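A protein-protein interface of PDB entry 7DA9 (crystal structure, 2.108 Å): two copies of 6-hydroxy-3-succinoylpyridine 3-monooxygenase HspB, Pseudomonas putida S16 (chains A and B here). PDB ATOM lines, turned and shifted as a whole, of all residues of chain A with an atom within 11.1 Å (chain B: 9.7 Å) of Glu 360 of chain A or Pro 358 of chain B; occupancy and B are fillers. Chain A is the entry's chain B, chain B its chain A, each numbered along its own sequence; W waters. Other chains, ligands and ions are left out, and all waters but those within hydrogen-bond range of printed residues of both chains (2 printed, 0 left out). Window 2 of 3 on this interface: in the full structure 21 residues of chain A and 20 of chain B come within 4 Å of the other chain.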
ATOM      1  N   VAL A 209      18.279 -31.041  12.195  1.00  0.00           N
ATOM      2  CA  VAL A 209      17.101 -30.953  11.342  1.00  0.00           C
ATOM      3  C   VAL A 209      17.471 -30.245  10.038  1.00  0.00           C
ATOM      4  O   VAL A 209      17.969 -29.107  10.052  1.00  0.00           O
ATOM      5  CB  VAL A 209      15.962 -30.227  12.071  1.00  0.00           C
ATOM      6  CG1 VAL A 209      14.770 -29.997  11.130  1.00  0.00           C
ATOM      7  CG2 VAL A 209      15.568 -31.026  13.308  1.00  0.00           C
ATOM      8  N   ASN A 352      10.190 -35.518  10.081  1.00  0.00           N
ATOM      9  CA  ASN A 352      10.479 -34.225  10.690  1.00  0.00           C
ATOM     10  C   ASN A 352      11.973 -33.936  10.680  1.00  0.00           C
ATOM     11  O   ASN A 352      12.382 -32.787  10.480  1.00  0.00           O
ATOM     12  CB  ASN A 352       9.934 -34.169  12.121  1.00  0.00           C
ATOM     13  CG  ASN A 352       8.417 -34.010  12.165  1.00  0.00           C
ATOM     14  OD1 ASN A 352       7.809 -33.428  11.262  1.00  0.00           O
ATOM     15  ND2 ASN A 352       7.806 -34.543  13.207  1.00  0.00           N
ATOM     16  N   HIS A 355      13.468 -34.495   6.218  1.00  0.00           N
ATOM     17  CA  HIS A 355      12.784 -34.135   4.972  1.00  0.00           C
ATOM     18  C   HIS A 355      12.044 -32.797   5.017  1.00  0.00           C
ATOM     19  O   HIS A 355      11.248 -32.524   4.112  1.00  0.00           O
ATOM     20  CB  HIS A 355      11.762 -35.225   4.555  1.00  0.00           C
ATOM     21  CG  HIS A 355      12.342 -36.600   4.404  1.00  0.00           C
ATOM     22  ND1 HIS A 355      13.522 -36.848   3.740  1.00  0.00           N
ATOM     23  CD2 HIS A 355      11.897 -37.806   4.836  1.00  0.00           C
ATOM     24  CE1 HIS A 355      13.788 -38.143   3.775  1.00  0.00           C
ATOM     25  NE2 HIS A 355      12.816 -38.747   4.434  1.00  0.00           N
ATOM     26  N   GLN A 356      12.222 -31.984   6.051  1.00  0.00           N
ATOM     27  CA  GLN A 356      11.533 -30.691   6.123  1.00  0.00           C
ATOM     28  C   GLN A 356      12.336 -29.664   5.330  1.00  0.00           C
ATOM     29  O   GLN A 356      13.377 -29.188   5.790  1.00  0.00           O
ATOM     30  CB  GLN A 356      11.375 -30.234   7.567  1.00  0.00           C
ATOM     31  CG  GLN A 356      10.370 -31.014   8.415  1.00  0.00           C
ATOM     32  CD  GLN A 356       9.975 -30.232   9.655  1.00  0.00           C
ATOM     33  OE1 GLN A 356       9.069 -29.401   9.608  1.00  0.00           O
ATOM     34  NE2 GLN A 356      10.676 -30.472  10.765  1.00  0.00           N
ATOM     35  N   LYS A 357      11.847 -29.314   4.132  1.00  0.00           N
ATOM     36  CA  LYS A 357      12.475 -28.311   3.288  1.00  0.00           C
ATOM     37  C   LYS A 357      12.134 -26.922   3.812  1.00  0.00           C
ATOM     38  O   LYS A 357      11.203 -26.768   4.605  1.00  0.00           O
ATOM     39  CB  LYS A 357      12.003 -28.478   1.844  1.00  0.00           C
ATOM     40  CG  LYS A 357      12.586 -29.700   1.104  1.00  0.00           C
ATOM     41  CD  LYS A 357      11.778 -30.000  -0.162  1.00  0.00           C
ATOM     42  CE  LYS A 357      12.358 -31.167  -0.969  1.00  0.00           C
ATOM     43  NZ  LYS A 357      11.585 -31.379  -2.232  1.00  0.00           N
ATOM     44  N   PRO A 358      12.881 -25.892   3.411  1.00  0.00           N
ATOM     45  CA  PRO A 358      12.565 -24.538   3.894  1.00  0.00           C
ATOM     46  C   PRO A 358      11.117 -24.163   3.589  1.00  0.00           C
ATOM     47  O   PRO A 358      10.569 -24.527   2.544  1.00  0.00           O
ATOM     48  CB  PRO A 358      13.556 -23.649   3.131  1.00  0.00           C
ATOM     49  CG  PRO A 358      14.720 -24.567   2.838  1.00  0.00           C
ATOM     50  CD  PRO A 358      14.119 -25.924   2.609  1.00  0.00           C
ATOM     51  N   GLY A 359      10.492 -23.449   4.516  1.00  0.00           N
ATOM     52  CA  GLY A 359       9.091 -23.113   4.354  1.00  0.00           C
ATOM     53  C   GLY A 359       8.405 -22.839   5.679  1.00  0.00           C
ATOM     54  O   GLY A 359       9.017 -22.849   6.746  1.00  0.00           O
ATOM     55  N   GLU A 360       7.099 -22.567   5.576  1.00  0.00           N
ATOM     56  CA  GLU A 360       6.312 -22.250   6.764  1.00  0.00           C
ATOM     57  C   GLU A 360       6.238 -23.432   7.714  1.00  0.00           C
ATOM     58  O   GLU A 360       6.268 -23.254   8.936  1.00  0.00           O
ATOM     59  CB  GLU A 360       4.905 -21.817   6.367  1.00  0.00           C
ATOM     60  CG  GLU A 360       4.603 -20.412   6.769  1.00  0.00           C
ATOM     61  CD  GLU A 360       3.451 -19.857   5.993  1.00  0.00           C
ATOM     62  OE1 GLU A 360       2.362 -20.472   6.052  1.00  0.00           O
ATOM     63  OE2 GLU A 360       3.647 -18.820   5.315  1.00  0.00           O
ATOM     64  N   GLY A 361       6.122 -24.645   7.169  1.00  0.00           N
ATOM     65  CA  GLY A 361       6.009 -25.823   8.015  1.00  0.00           C
ATOM     66  C   GLY A 361       7.219 -26.002   8.911  1.00  0.00           C
ATOM     67  O   GLY A 361       7.087 -26.255  10.109  1.00  0.00           O
ATOM     68  N   LYS A 362       8.414 -25.838   8.349  1.00  0.00           N
ATOM     69  CA  LYS A 362       9.622 -25.992   9.154  1.00  0.00           C
ATOM     70  C   LYS A 362       9.762 -24.872  10.180  1.00  0.00           C
ATOM     71  O   LYS A 362      10.187 -25.119  11.315  1.00  0.00           O
ATOM     72  CB  LYS A 362      10.846 -26.050   8.246  1.00  0.00           C
ATOM     73  CG  LYS A 362      12.173 -26.034   8.995  1.00  0.00           C
ATOM     74  CD  LYS A 362      13.303 -25.670   8.059  1.00  0.00           C
ATOM     75  CE  LYS A 362      14.663 -26.034   8.631  1.00  0.00           C
ATOM     76  NZ  LYS A 362      15.711 -25.700   7.609  1.00  0.00           N
ATOM     77  N   ASN A 363       9.439 -23.629   9.797  1.00  0.00           N
ATOM     78  CA  ASN A 363       9.463 -22.524  10.755  1.00  0.00           C
ATOM     79  C   ASN A 363       8.491 -22.780  11.899  1.00  0.00           C
ATOM     80  O   ASN A 363       8.821 -22.541  13.072  1.00  0.00           O
ATOM     81  CB  ASN A 363       9.112 -21.204  10.071  1.00  0.00           C
ATOM     82  CG  ASN A 363      10.135 -20.773   9.028  1.00  0.00           C
ATOM     83  OD1 ASN A 363      11.262 -21.282   8.962  1.00  0.00           O
ATOM     84  ND2 ASN A 363       9.745 -19.801   8.220  1.00  0.00           N
ATOM     85  N   ASP A 364       7.281 -23.261  11.570  1.00  0.00           N
ATOM     86  CA  ASP A 364       6.329 -23.701  12.589  1.00  0.00           C
ATOM     87  C   ASP A 364       6.924 -24.793  13.464  1.00  0.00           C
ATOM     88  O   ASP A 364       6.762 -24.779  14.693  1.00  0.00           O
ATOM     89  CB  ASP A 364       5.056 -24.235  11.933  1.00  0.00           C
ATOM     90  CG  ASP A 364       4.156 -23.142  11.402  1.00  0.00           C
ATOM     91  OD1 ASP A 364       4.492 -21.946  11.557  1.00  0.00           O
ATOM     92  OD2 ASP A 364       3.099 -23.501  10.828  1.00  0.00           O
ATOM     93  N   TRP A 365       7.581 -25.777  12.845  1.00  0.00           N
ATOM     94  CA  TRP A 365       8.178 -26.848  13.634  1.00  0.00           C
ATOM     95  C   TRP A 365       9.197 -26.285  14.619  1.00  0.00           C
ATOM     96  O   TRP A 365       9.183 -26.626  15.808  1.00  0.00           O
ATOM     97  CB  TRP A 365       8.832 -27.892  12.721  1.00  0.00           C
ATOM     98  CG  TRP A 365       9.328 -29.067  13.507  1.00  0.00           C
ATOM     99  CD1 TRP A 365       8.638 -30.220  13.786  1.00  0.00           C
ATOM    100  CD2 TRP A 365      10.597 -29.195  14.161  1.00  0.00           C
ATOM    101  NE1 TRP A 365       9.414 -31.061  14.556  1.00  0.00           N
ATOM    102  CE2 TRP A 365      10.619 -30.459  14.795  1.00  0.00           C
ATOM    103  CE3 TRP A 365      11.726 -28.377  14.249  1.00  0.00           C
ATOM    104  CZ2 TRP A 365      11.716 -30.913  15.516  1.00  0.00           C
ATOM    105  CZ3 TRP A 365      12.816 -28.829  14.970  1.00  0.00           C
ATOM    106  CH2 TRP A 365      12.803 -30.086  15.591  1.00  0.00           C
ATOM    107  N   VAL A 366      10.077 -25.403  14.147  1.00  0.00           N
ATOM    108  CA  VAL A 366      11.146 -24.899  15.013  1.00  0.00           C
ATOM    109  C   VAL A 366      10.565 -24.076  16.164  1.00  0.00           C
ATOM    110  O   VAL A 366      10.971 -24.231  17.322  1.00  0.00           O
ATOM    111  CB  VAL A 366      12.166 -24.100  14.180  1.00  0.00           C
ATOM    112  CG1 VAL A 366      13.196 -23.390  15.082  1.00  0.00           C
ATOM    113  CG2 VAL A 366      12.854 -25.021  13.180  1.00  0.00           C
ATOM    114  N   ASN A 367       9.587 -23.215  15.868  1.00  0.00           N
ATOM    115  CA  ASN A 367       8.975 -22.377  16.897  1.00  0.00           C
ATOM    116  C   ASN A 367       8.273 -23.213  17.966  1.00  0.00           C
ATOM    117  O   ASN A 367       8.314 -22.879  19.157  1.00  0.00           O
ATOM    118  CB  ASN A 367       7.996 -21.404  16.250  1.00  0.00           C
ATOM    119  CG  ASN A 367       8.689 -20.383  15.368  1.00  0.00           C
ATOM    120  OD1 ASN A 367       9.865 -20.078  15.560  1.00  0.00           O
ATOM    121  ND2 ASN A 367       7.964 -19.853  14.391  1.00  0.00           N
ATOM    122  N   ASN A 368       7.625 -24.304  17.562  1.00  0.00           N
ATOM    123  CA  ASN A 368       6.978 -25.173  18.538  1.00  0.00           C
ATOM    124  C   ASN A 368       8.007 -25.893  19.404  1.00  0.00           C
ATOM    125  O   ASN A 368       7.887 -25.922  20.633  1.00  0.00           O
ATOM    126  CB  ASN A 368       6.079 -26.181  17.821  1.00  0.00           C
ATOM    127  CG  ASN A 368       5.157 -26.886  18.770  1.00  0.00           C
ATOM    128  OD1 ASN A 368       4.494 -26.247  19.593  1.00  0.00           O
ATOM    129  ND2 ASN A 368       5.118 -28.209  18.687  1.00  0.00           N
ATOM    130  N   THR A 369       9.016 -26.498  18.771  1.00  0.00           N
ATOM    131  CA  THR A 369      10.115 -27.118  19.504  1.00  0.00           C
ATOM    132  C   THR A 369      10.744 -26.150  20.506  1.00  0.00           C
ATOM    133  O   THR A 369      11.092 -26.538  21.629  1.00  0.00           O
ATOM    134  CB  THR A 369      11.166 -27.612  18.514  1.00  0.00           C
ATOM    135  OG1 THR A 369      10.543 -28.446  17.528  1.00  0.00           O
ATOM    136  CG2 THR A 369      12.272 -28.371  19.235  1.00  0.00           C
ATOM    137  N   ARG A 370      10.895 -24.881  20.123  1.00  0.00           N
ATOM    138  CA  ARG A 370      11.484 -23.910  21.044  1.00  0.00           C
ATOM    139  C   ARG A 370      10.510 -23.540  22.155  1.00  0.00           C
ATOM    140  O   ARG A 370      10.920 -23.310  23.300  1.00  0.00           O
ATOM    141  CB  ARG A 370      11.931 -22.653  20.291  1.00  0.00           C
ATOM    142  CG  ARG A 370      13.031 -21.835  21.019  1.00  0.00           C
ATOM    143  CD  ARG A 370      13.532 -20.685  20.144  1.00  0.00           C
ATOM    144  NE  ARG A 370      12.451 -20.206  19.291  1.00  0.00           N
ATOM    145  CZ  ARG A 370      12.509 -20.078  17.968  1.00  0.00           C
ATOM    146  NH1 ARG A 370      13.621 -20.364  17.302  1.00  0.00           N
ATOM    147  NH2 ARG A 370      11.438 -19.651  17.307  1.00  0.00           N
ATOM    148  N   VAL B  79      -4.010 -25.272  -7.782  1.00  0.00           N
ATOM    149  CA  VAL B  79      -3.223 -24.685  -6.702  1.00  0.00           C
ATOM    150  C   VAL B  79      -3.985 -23.468  -6.183  1.00  0.00           C
ATOM    151  O   VAL B  79      -4.180 -22.485  -6.909  1.00  0.00           O
ATOM    152  CB  VAL B  79      -1.809 -24.313  -7.155  1.00  0.00           C
ATOM    153  CG1 VAL B  79      -1.011 -23.820  -5.953  1.00  0.00           C
ATOM    154  CG2 VAL B  79      -1.130 -25.527  -7.817  1.00  0.00           C
ATOM    155  N   HIS B  80      -4.421 -23.542  -4.922  1.00  0.00           N
ATOM    156  CA  HIS B  80      -5.266 -22.489  -4.372  1.00  0.00           C
ATOM    157  C   HIS B  80      -4.517 -21.164  -4.297  1.00  0.00           C
ATOM    158  O   HIS B  80      -5.078 -20.115  -4.611  1.00  0.00           O
ATOM    159  CB  HIS B  80      -5.785 -22.900  -2.995  1.00  0.00           C
ATOM    160  CG  HIS B  80      -6.734 -21.915  -2.378  1.00  0.00           C
ATOM    161  ND1 HIS B  80      -8.069 -21.852  -2.716  1.00  0.00           N
ATOM    162  CD2 HIS B  80      -6.540 -20.959  -1.437  1.00  0.00           C
ATOM    163  CE1 HIS B  80      -8.658 -20.907  -2.005  1.00  0.00           C
ATOM    164  NE2 HIS B  80      -7.750 -20.344  -1.227  1.00  0.00           N
ATOM    165  N   SER B  81      -3.239 -21.198  -3.936  1.00  0.00           N
ATOM    166  CA  SER B  81      -2.499 -19.948  -3.762  1.00  0.00           C
ATOM    167  C   SER B  81      -2.370 -19.173  -5.066  1.00  0.00           C
ATOM    168  O   SER B  81      -2.346 -17.941  -5.044  1.00  0.00           O
ATOM    169  CB  SER B  81      -1.121 -20.229  -3.176  1.00  0.00           C
ATOM    170  OG  SER B  81      -0.424 -21.177  -3.973  1.00  0.00           O
ATOM    171  N   VAL B 209      -5.260 -28.016  -3.951  1.00  0.00           N
ATOM    172  CA  VAL B 209      -4.123 -28.148  -3.040  1.00  0.00           C
ATOM    173  C   VAL B 209      -3.943 -26.863  -2.247  1.00  0.00           C
ATOM    174  O   VAL B 209      -3.788 -25.779  -2.831  1.00  0.00           O
ATOM    175  CB  VAL B 209      -2.838 -28.490  -3.814  1.00  0.00           C
ATOM    176  CG1 VAL B 209      -1.604 -28.442  -2.910  1.00  0.00           C
ATOM    177  CG2 VAL B 209      -2.995 -29.839  -4.478  1.00  0.00           C
ATOM    178  N   ASP B 210      -3.934 -26.984  -0.921  1.00  0.00           N
ATOM    179  CA  ASP B 210      -3.709 -25.869  -0.003  1.00  0.00           C
ATOM    180  C   ASP B 210      -3.476 -26.461   1.378  1.00  0.00           C
ATOM    181  O   ASP B 210      -3.700 -27.651   1.604  1.00  0.00           O
ATOM    182  CB  ASP B 210      -4.888 -24.885   0.050  1.00  0.00           C
ATOM    183  CG  ASP B 210      -4.519 -23.561   0.730  1.00  0.00           C
ATOM    184  OD1 ASP B 210      -3.639 -22.839   0.196  1.00  0.00           O
ATOM    185  OD2 ASP B 210      -5.103 -23.253   1.806  1.00  0.00           O
ATOM    186  N   ASP B 211      -3.039 -25.619   2.310  1.00  0.00           N
ATOM    187  CA  ASP B 211      -2.918 -26.094   3.675  1.00  0.00           C
ATOM    188  C   ASP B 211      -4.112 -25.728   4.557  1.00  0.00           C
ATOM    189  O   ASP B 211      -4.290 -26.336   5.622  1.00  0.00           O
ATOM    190  CB  ASP B 211      -1.615 -25.578   4.294  1.00  0.00           C
ATOM    191  CG  ASP B 211      -1.597 -24.079   4.430  1.00  0.00           C
ATOM    192  OD1 ASP B 211      -1.430 -23.615   5.572  1.00  0.00           O
ATOM    193  OD2 ASP B 211      -1.769 -23.372   3.406  1.00  0.00           O
ATOM    194  N   VAL B 212      -4.951 -24.783   4.153  1.00  0.00           N
ATOM    195  CA  VAL B 212      -6.188 -24.487   4.871  1.00  0.00           C
ATOM    196  C   VAL B 212      -7.405 -24.921   4.063  1.00  0.00           C
ATOM    197  O   VAL B 212      -8.311 -25.564   4.586  1.00  0.00           O
ATOM    198  CB  VAL B 212      -6.281 -22.990   5.242  1.00  0.00           C
ATOM    199  CG1 VAL B 212      -7.603 -22.703   5.932  1.00  0.00           C
ATOM    200  CG2 VAL B 212      -5.086 -22.546   6.128  1.00  0.00           C
ATOM    201  N   TYR B 354      -3.919 -31.694   1.443  1.00  0.00           N
ATOM    202  CA  TYR B 354      -4.474 -30.891   2.531  1.00  0.00           C
ATOM    203  C   TYR B 354      -3.449 -30.243   3.458  1.00  0.00           C
ATOM    204  O   TYR B 354      -3.845 -29.432   4.298  1.00  0.00           O
ATOM    205  CB  TYR B 354      -5.400 -31.749   3.404  1.00  0.00           C
ATOM    206  CG  TYR B 354      -6.646 -32.247   2.718  1.00  0.00           C
ATOM    207  CD1 TYR B 354      -6.722 -33.541   2.234  1.00  0.00           C
ATOM    208  CD2 TYR B 354      -7.754 -31.419   2.561  1.00  0.00           C
ATOM    209  CE1 TYR B 354      -7.868 -34.009   1.611  1.00  0.00           C
ATOM    210  CE2 TYR B 354      -8.903 -31.871   1.942  1.00  0.00           C
ATOM    211  CZ  TYR B 354      -8.957 -33.175   1.471  1.00  0.00           C
ATOM    212  OH  TYR B 354     -10.100 -33.639   0.850  1.00  0.00           O
ATOM    213  N   HIS B 355      -2.159 -30.569   3.356  1.00  0.00           N
ATOM    214  CA  HIS B 355      -1.249 -30.254   4.450  1.00  0.00           C
ATOM    215  C   HIS B 355       0.061 -29.599   4.019  1.00  0.00           C
ATOM    216  O   HIS B 355       0.959 -29.450   4.856  1.00  0.00           O
ATOM    217  CB  HIS B 355      -0.945 -31.519   5.265  1.00  0.00           C
ATOM    218  CG  HIS B 355      -2.105 -31.990   6.086  1.00  0.00           C
ATOM    219  ND1 HIS B 355      -2.231 -33.294   6.521  1.00  0.00           N
ATOM    220  CD2 HIS B 355      -3.196 -31.333   6.544  1.00  0.00           C
ATOM    221  CE1 HIS B 355      -3.351 -33.418   7.210  1.00  0.00           C
ATOM    222  NE2 HIS B 355      -3.959 -32.245   7.230  1.00  0.00           N
ATOM    223  N   GLN B 356       0.202 -29.190   2.762  1.00  0.00           N
ATOM    224  CA  GLN B 356       1.420 -28.507   2.314  1.00  0.00           C
ATOM    225  C   GLN B 356       1.292 -27.007   2.560  1.00  0.00           C
ATOM    226  O   GLN B 356       0.573 -26.309   1.839  1.00  0.00           O
ATOM    227  CB  GLN B 356       1.710 -28.780   0.840  1.00  0.00           C
ATOM    228  CG  GLN B 356       2.009 -30.246   0.523  1.00  0.00           C
ATOM    229  CD  GLN B 356       2.515 -30.400  -0.888  1.00  0.00           C
ATOM    230  OE1 GLN B 356       3.667 -30.075  -1.172  1.00  0.00           O
ATOM    231  NE2 GLN B 356       1.637 -30.846  -1.800  1.00  0.00           N
ATOM    232  N   LYS B 357       2.010 -26.516   3.570  1.00  0.00           N
ATOM    233  CA  LYS B 357       2.146 -25.091   3.791  1.00  0.00           C
ATOM    234  C   LYS B 357       3.118 -24.495   2.772  1.00  0.00           C
ATOM    235  O   LYS B 357       3.857 -25.226   2.108  1.00  0.00           O
ATOM    236  CB  LYS B 357       2.628 -24.844   5.215  1.00  0.00           C
ATOM    237  CG  LYS B 357       1.588 -25.216   6.282  1.00  0.00           C
ATOM    238  CD  LYS B 357       2.302 -25.638   7.561  1.00  0.00           C
ATOM    239  CE  LYS B 357       1.407 -25.567   8.786  1.00  0.00           C
ATOM    240  NZ  LYS B 357       2.222 -25.713  10.030  1.00  0.00           N
ATOM    241  N   PRO B 358       3.108 -23.171   2.597  1.00  0.00           N
ATOM    242  CA  PRO B 358       4.039 -22.554   1.641  1.00  0.00           C
ATOM    243  C   PRO B 358       5.487 -22.918   1.941  1.00  0.00           C
ATOM    244  O   PRO B 358       5.882 -23.048   3.101  1.00  0.00           O
ATOM    245  CB  PRO B 358       3.796 -21.052   1.824  1.00  0.00           C
ATOM    246  CG  PRO B 358       2.399 -20.965   2.323  1.00  0.00           C
ATOM    247  CD  PRO B 358       2.137 -22.198   3.127  1.00  0.00           C
ATOM    248  N   GLY B 359       6.273 -23.077   0.882  1.00  0.00           N
ATOM    249  CA  GLY B 359       7.678 -23.401   1.026  1.00  0.00           C
ATOM    250  C   GLY B 359       8.223 -24.100  -0.208  1.00  0.00           C
ATOM    251  O   GLY B 359       7.574 -24.167  -1.260  1.00  0.00           O
ATOM    252  N   GLU B 360       9.448 -24.611  -0.052  1.00  0.00           N
ATOM    253  CA  GLU B 360      10.120 -25.283  -1.160  1.00  0.00           C
ATOM    254  C   GLU B 360       9.400 -26.567  -1.543  1.00  0.00           C
ATOM    255  O   GLU B 360       9.224 -26.840  -2.733  1.00  0.00           O
ATOM    256  CB  GLU B 360      11.585 -25.569  -0.808  1.00  0.00           C
ATOM    257  CG  GLU B 360      12.548 -24.440  -1.221  1.00  0.00           C
ATOM    258  CD  GLU B 360      14.022 -24.777  -0.979  1.00  0.00           C
ATOM    259  OE1 GLU B 360      14.343 -25.957  -0.718  1.00  0.00           O
ATOM    260  OE2 GLU B 360      14.858 -23.846  -1.031  1.00  0.00           O
ATOM    261  N   GLY B 361       8.989 -27.368  -0.546  1.00  0.00           N
ATOM    262  CA  GLY B 361       8.274 -28.604  -0.828  1.00  0.00           C
ATOM    263  C   GLY B 361       7.069 -28.406  -1.735  1.00  0.00           C
ATOM    264  O   GLY B 361       6.926 -29.076  -2.760  1.00  0.00           O
ATOM    265  N   LYS B 362       6.190 -27.469  -1.379  1.00  0.00           N
ATOM    266  CA  LYS B 362       4.996 -27.236  -2.187  1.00  0.00           C
ATOM    267  C   LYS B 362       5.359 -26.791  -3.601  1.00  0.00           C
ATOM    268  O   LYS B 362       4.759 -27.254  -4.582  1.00  0.00           O
ATOM    269  CB  LYS B 362       4.102 -26.203  -1.500  1.00  0.00           C
ATOM    270  CG  LYS B 362       2.728 -26.013  -2.127  1.00  0.00           C
ATOM    271  CD  LYS B 362       2.153 -24.652  -1.741  1.00  0.00           C
ATOM    272  CE  LYS B 362       0.709 -24.471  -2.193  1.00  0.00           C
ATOM    273  NZ  LYS B 362       0.161 -23.217  -1.585  1.00  0.00           N
ATOM    274  N   ASN B 363       6.343 -25.898  -3.732  1.00  0.00           N
ATOM    275  CA  ASN B 363       6.760 -25.458  -5.060  1.00  0.00           C
ATOM    276  C   ASN B 363       7.320 -26.617  -5.875  1.00  0.00           C
ATOM    277  O   ASN B 363       7.075 -26.714  -7.084  1.00  0.00           O
ATOM    278  CB  ASN B 363       7.802 -24.340  -4.950  1.00  0.00           C
ATOM    279  CG  ASN B 363       7.281 -23.130  -4.206  1.00  0.00           C
ATOM    280  OD1 ASN B 363       6.066 -22.950  -4.059  1.00  0.00           O
ATOM    281  ND2 ASN B 363       8.202 -22.285  -3.729  1.00  0.00           N
ATOM    282  N   ASP B 364       8.082 -27.502  -5.234  1.00  0.00           N
ATOM    283  CA  ASP B 364       8.597 -28.673  -5.936  1.00  0.00           C
ATOM    284  C   ASP B 364       7.463 -29.594  -6.365  1.00  0.00           C
ATOM    285  O   ASP B 364       7.462 -30.102  -7.496  1.00  0.00           O
ATOM    286  CB  ASP B 364       9.568 -29.431  -5.041  1.00  0.00           C
ATOM    287  CG  ASP B 364      10.869 -28.694  -4.826  1.00  0.00           C
ATOM    288  OD1 ASP B 364      11.150 -27.721  -5.566  1.00  0.00           O
ATOM    289  OD2 ASP B 364      11.619 -29.116  -3.915  1.00  0.00           O
ATOM    290  N   VAL B 366       4.353 -28.776  -7.072  1.00  0.00           N
ATOM    291  CA  VAL B 366       3.643 -28.173  -8.206  1.00  0.00           C
ATOM    292  C   VAL B 366       4.476 -28.271  -9.488  1.00  0.00           C
ATOM    293  O   VAL B 366       3.984 -28.691 -10.539  1.00  0.00           O
ATOM    294  CB  VAL B 366       3.263 -26.710  -7.889  1.00  0.00           C
ATOM    295  CG1 VAL B 366       2.635 -26.030  -9.093  1.00  0.00           C
ATOM    296  CG2 VAL B 366       2.312 -26.648  -6.706  1.00  0.00           C
HETATM  297  O   HOH W   1       6.139 -25.507   4.512  1.00  0.00           O
HETATM  298  O   HOH W   2       8.782 -26.704   2.245  1.00  0.00           O
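The side-chain amino group (NZ) of Lys 357 of chain B is in salt-bridge range of the side-chain carboxylate (OD2) of Asp 364 of chain A (2.5 Å). The backbone carbonyl oxygen (O) of Pro 358 of chain B lies within hydrogen-bond range of the backbone NH (N) of Glu 360 of chain A, at 2.8 Å. O of Pro 358 of chain A lies within hydrogen-bond range of N of Glu 360 of chain B, 2.8 Å away. The side-chain carboxylate of Asp 364 of chain B is in salt-bridge range of the side-chain amino group of Lys 357 of chain A (2.8 Å).
ND2 of Asn 363 of chain B lies close to O of Gly 359 of chain B, 3.2 Å away. O of Gly 359 of chain A sits close to ND2 of Asn 363 of chain A, at 3.5 Å.
Among the printed residues, pairs that only touch across the chains: Gly 359 of chain A with Pro 358 of chain B (3.4 Å), Pro 358 of chain A with Gly 359 of chain B (3.5 Å), Gly 359 of chain A with Gly 359 of chain B (3.6 Å), Gly 361 of chain A with Lys 357 of chain B (3.7 Å), Lys 357 of chain A with Gly 361 of chain B (3.8 Å), Lys 357 of chain A with Glu 360 of chain B (3.96 Å) and Glu 360 of chain A with Lys 357 of chain B (3.96 Å).
Of chain B, only Lys 357 (3.96 Å) and Pro 358 (2.8 Å) come within 4 Å of Glu 360 of chain A. Of chain A, only Gly 359 and Glu 360 come within 4 Å of Pro 358 of chain B. Of the printed residues of chain B, Gly 361 of chain A touches Lys 357 (3.7 Å). No residue of chain B comes within 4 Å of Asn 363 of chain A. Of chain A, only Glu 360 (3.96 Å), Gly 361 (3.7 Å) and Asp 364 (2.5 Å) come within 4 Å of Lys 357 of chain B. Of the printed residues of chain B, Pro 358 of chain A touches Gly 359 and Glu 360. Printed residues of chain B within 4 Å of Lys 357 of chain A: Glu 360 (3.96 Å), Gly 361 (3.8 Å) and Asp 364 (2.8 Å). Of the printed residues of chain A, Gly 361 of chain B touches Lys 357. Trp 365 of chain A touches none of the printed residues of chain B. The nearest residue of chain A that does not touch Pro 358 of chain B is Gly 361 of chain A (4.4 Å). The nearest printed residue of chain B that does not touch Lys 357 of chain A is Gly 359 of chain B (6.0 Å).
Printed residues of chain B that touch a printed residue of chain A: Lys 357, Pro 358, Gly 359, Glu 360, Gly 361 and Asp 364. Hydrophobic or aromatic side chains of chain A within 4 Å of the printed part of chain B: Pro 358. Among the printed residues, 11 pairs touch across the chains. Among the printed residues, Asp or Glu carboxylates within 4 Å of a Lys or Arg side-chain nitrogen of the other chain: Lys 357 of chain A with Asp 364 of chain B and Asp 364 of chain A with Lys 357 of chain B.
Lys 357 of chain A touches Glu 360 of chain B, and with the chains exchanged Glu 360 of chain A touches Lys 357 of chain B. Lys 357 of chain A touches Gly 361 of chain B, and with the chains exchanged Gly 361 of chain A touches Lys 357 of chain B. Lys 357 of chain A touches Asp 364 of chain B, and with the chains exchanged Asp 364 of chain A touches Lys 357 of chain B. Pro 358 of chain A touches Gly 359 of chain B, and with the chains exchanged Gly 359 of chain A touches Pro 358 of chain B. 12 positions are printed for both chains. Of the 11 pairs that touch across the chains among the printed residues, 11 have their exchanged pair printed and touching as well.
Water W1 lies within hydrogen-bond range of the backbone NH (N) of Gly 361 of chain A (2.8 Å), the backbone carbonyl oxygen (O) of Pro 358 of chain B (2.8 Å), the backbone NH (N) of Glu 360 of chain A (3.3 Å) and the backbone carbonyl oxygen (O) of Lys 357 of chain B (3.3 Å). Water W2 lies within hydrogen-bond range of O of Pro 358 of chain A, N of Gly 361 of chain B, N of Glu 360 of chain B and O of Lys 357 of chain A.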
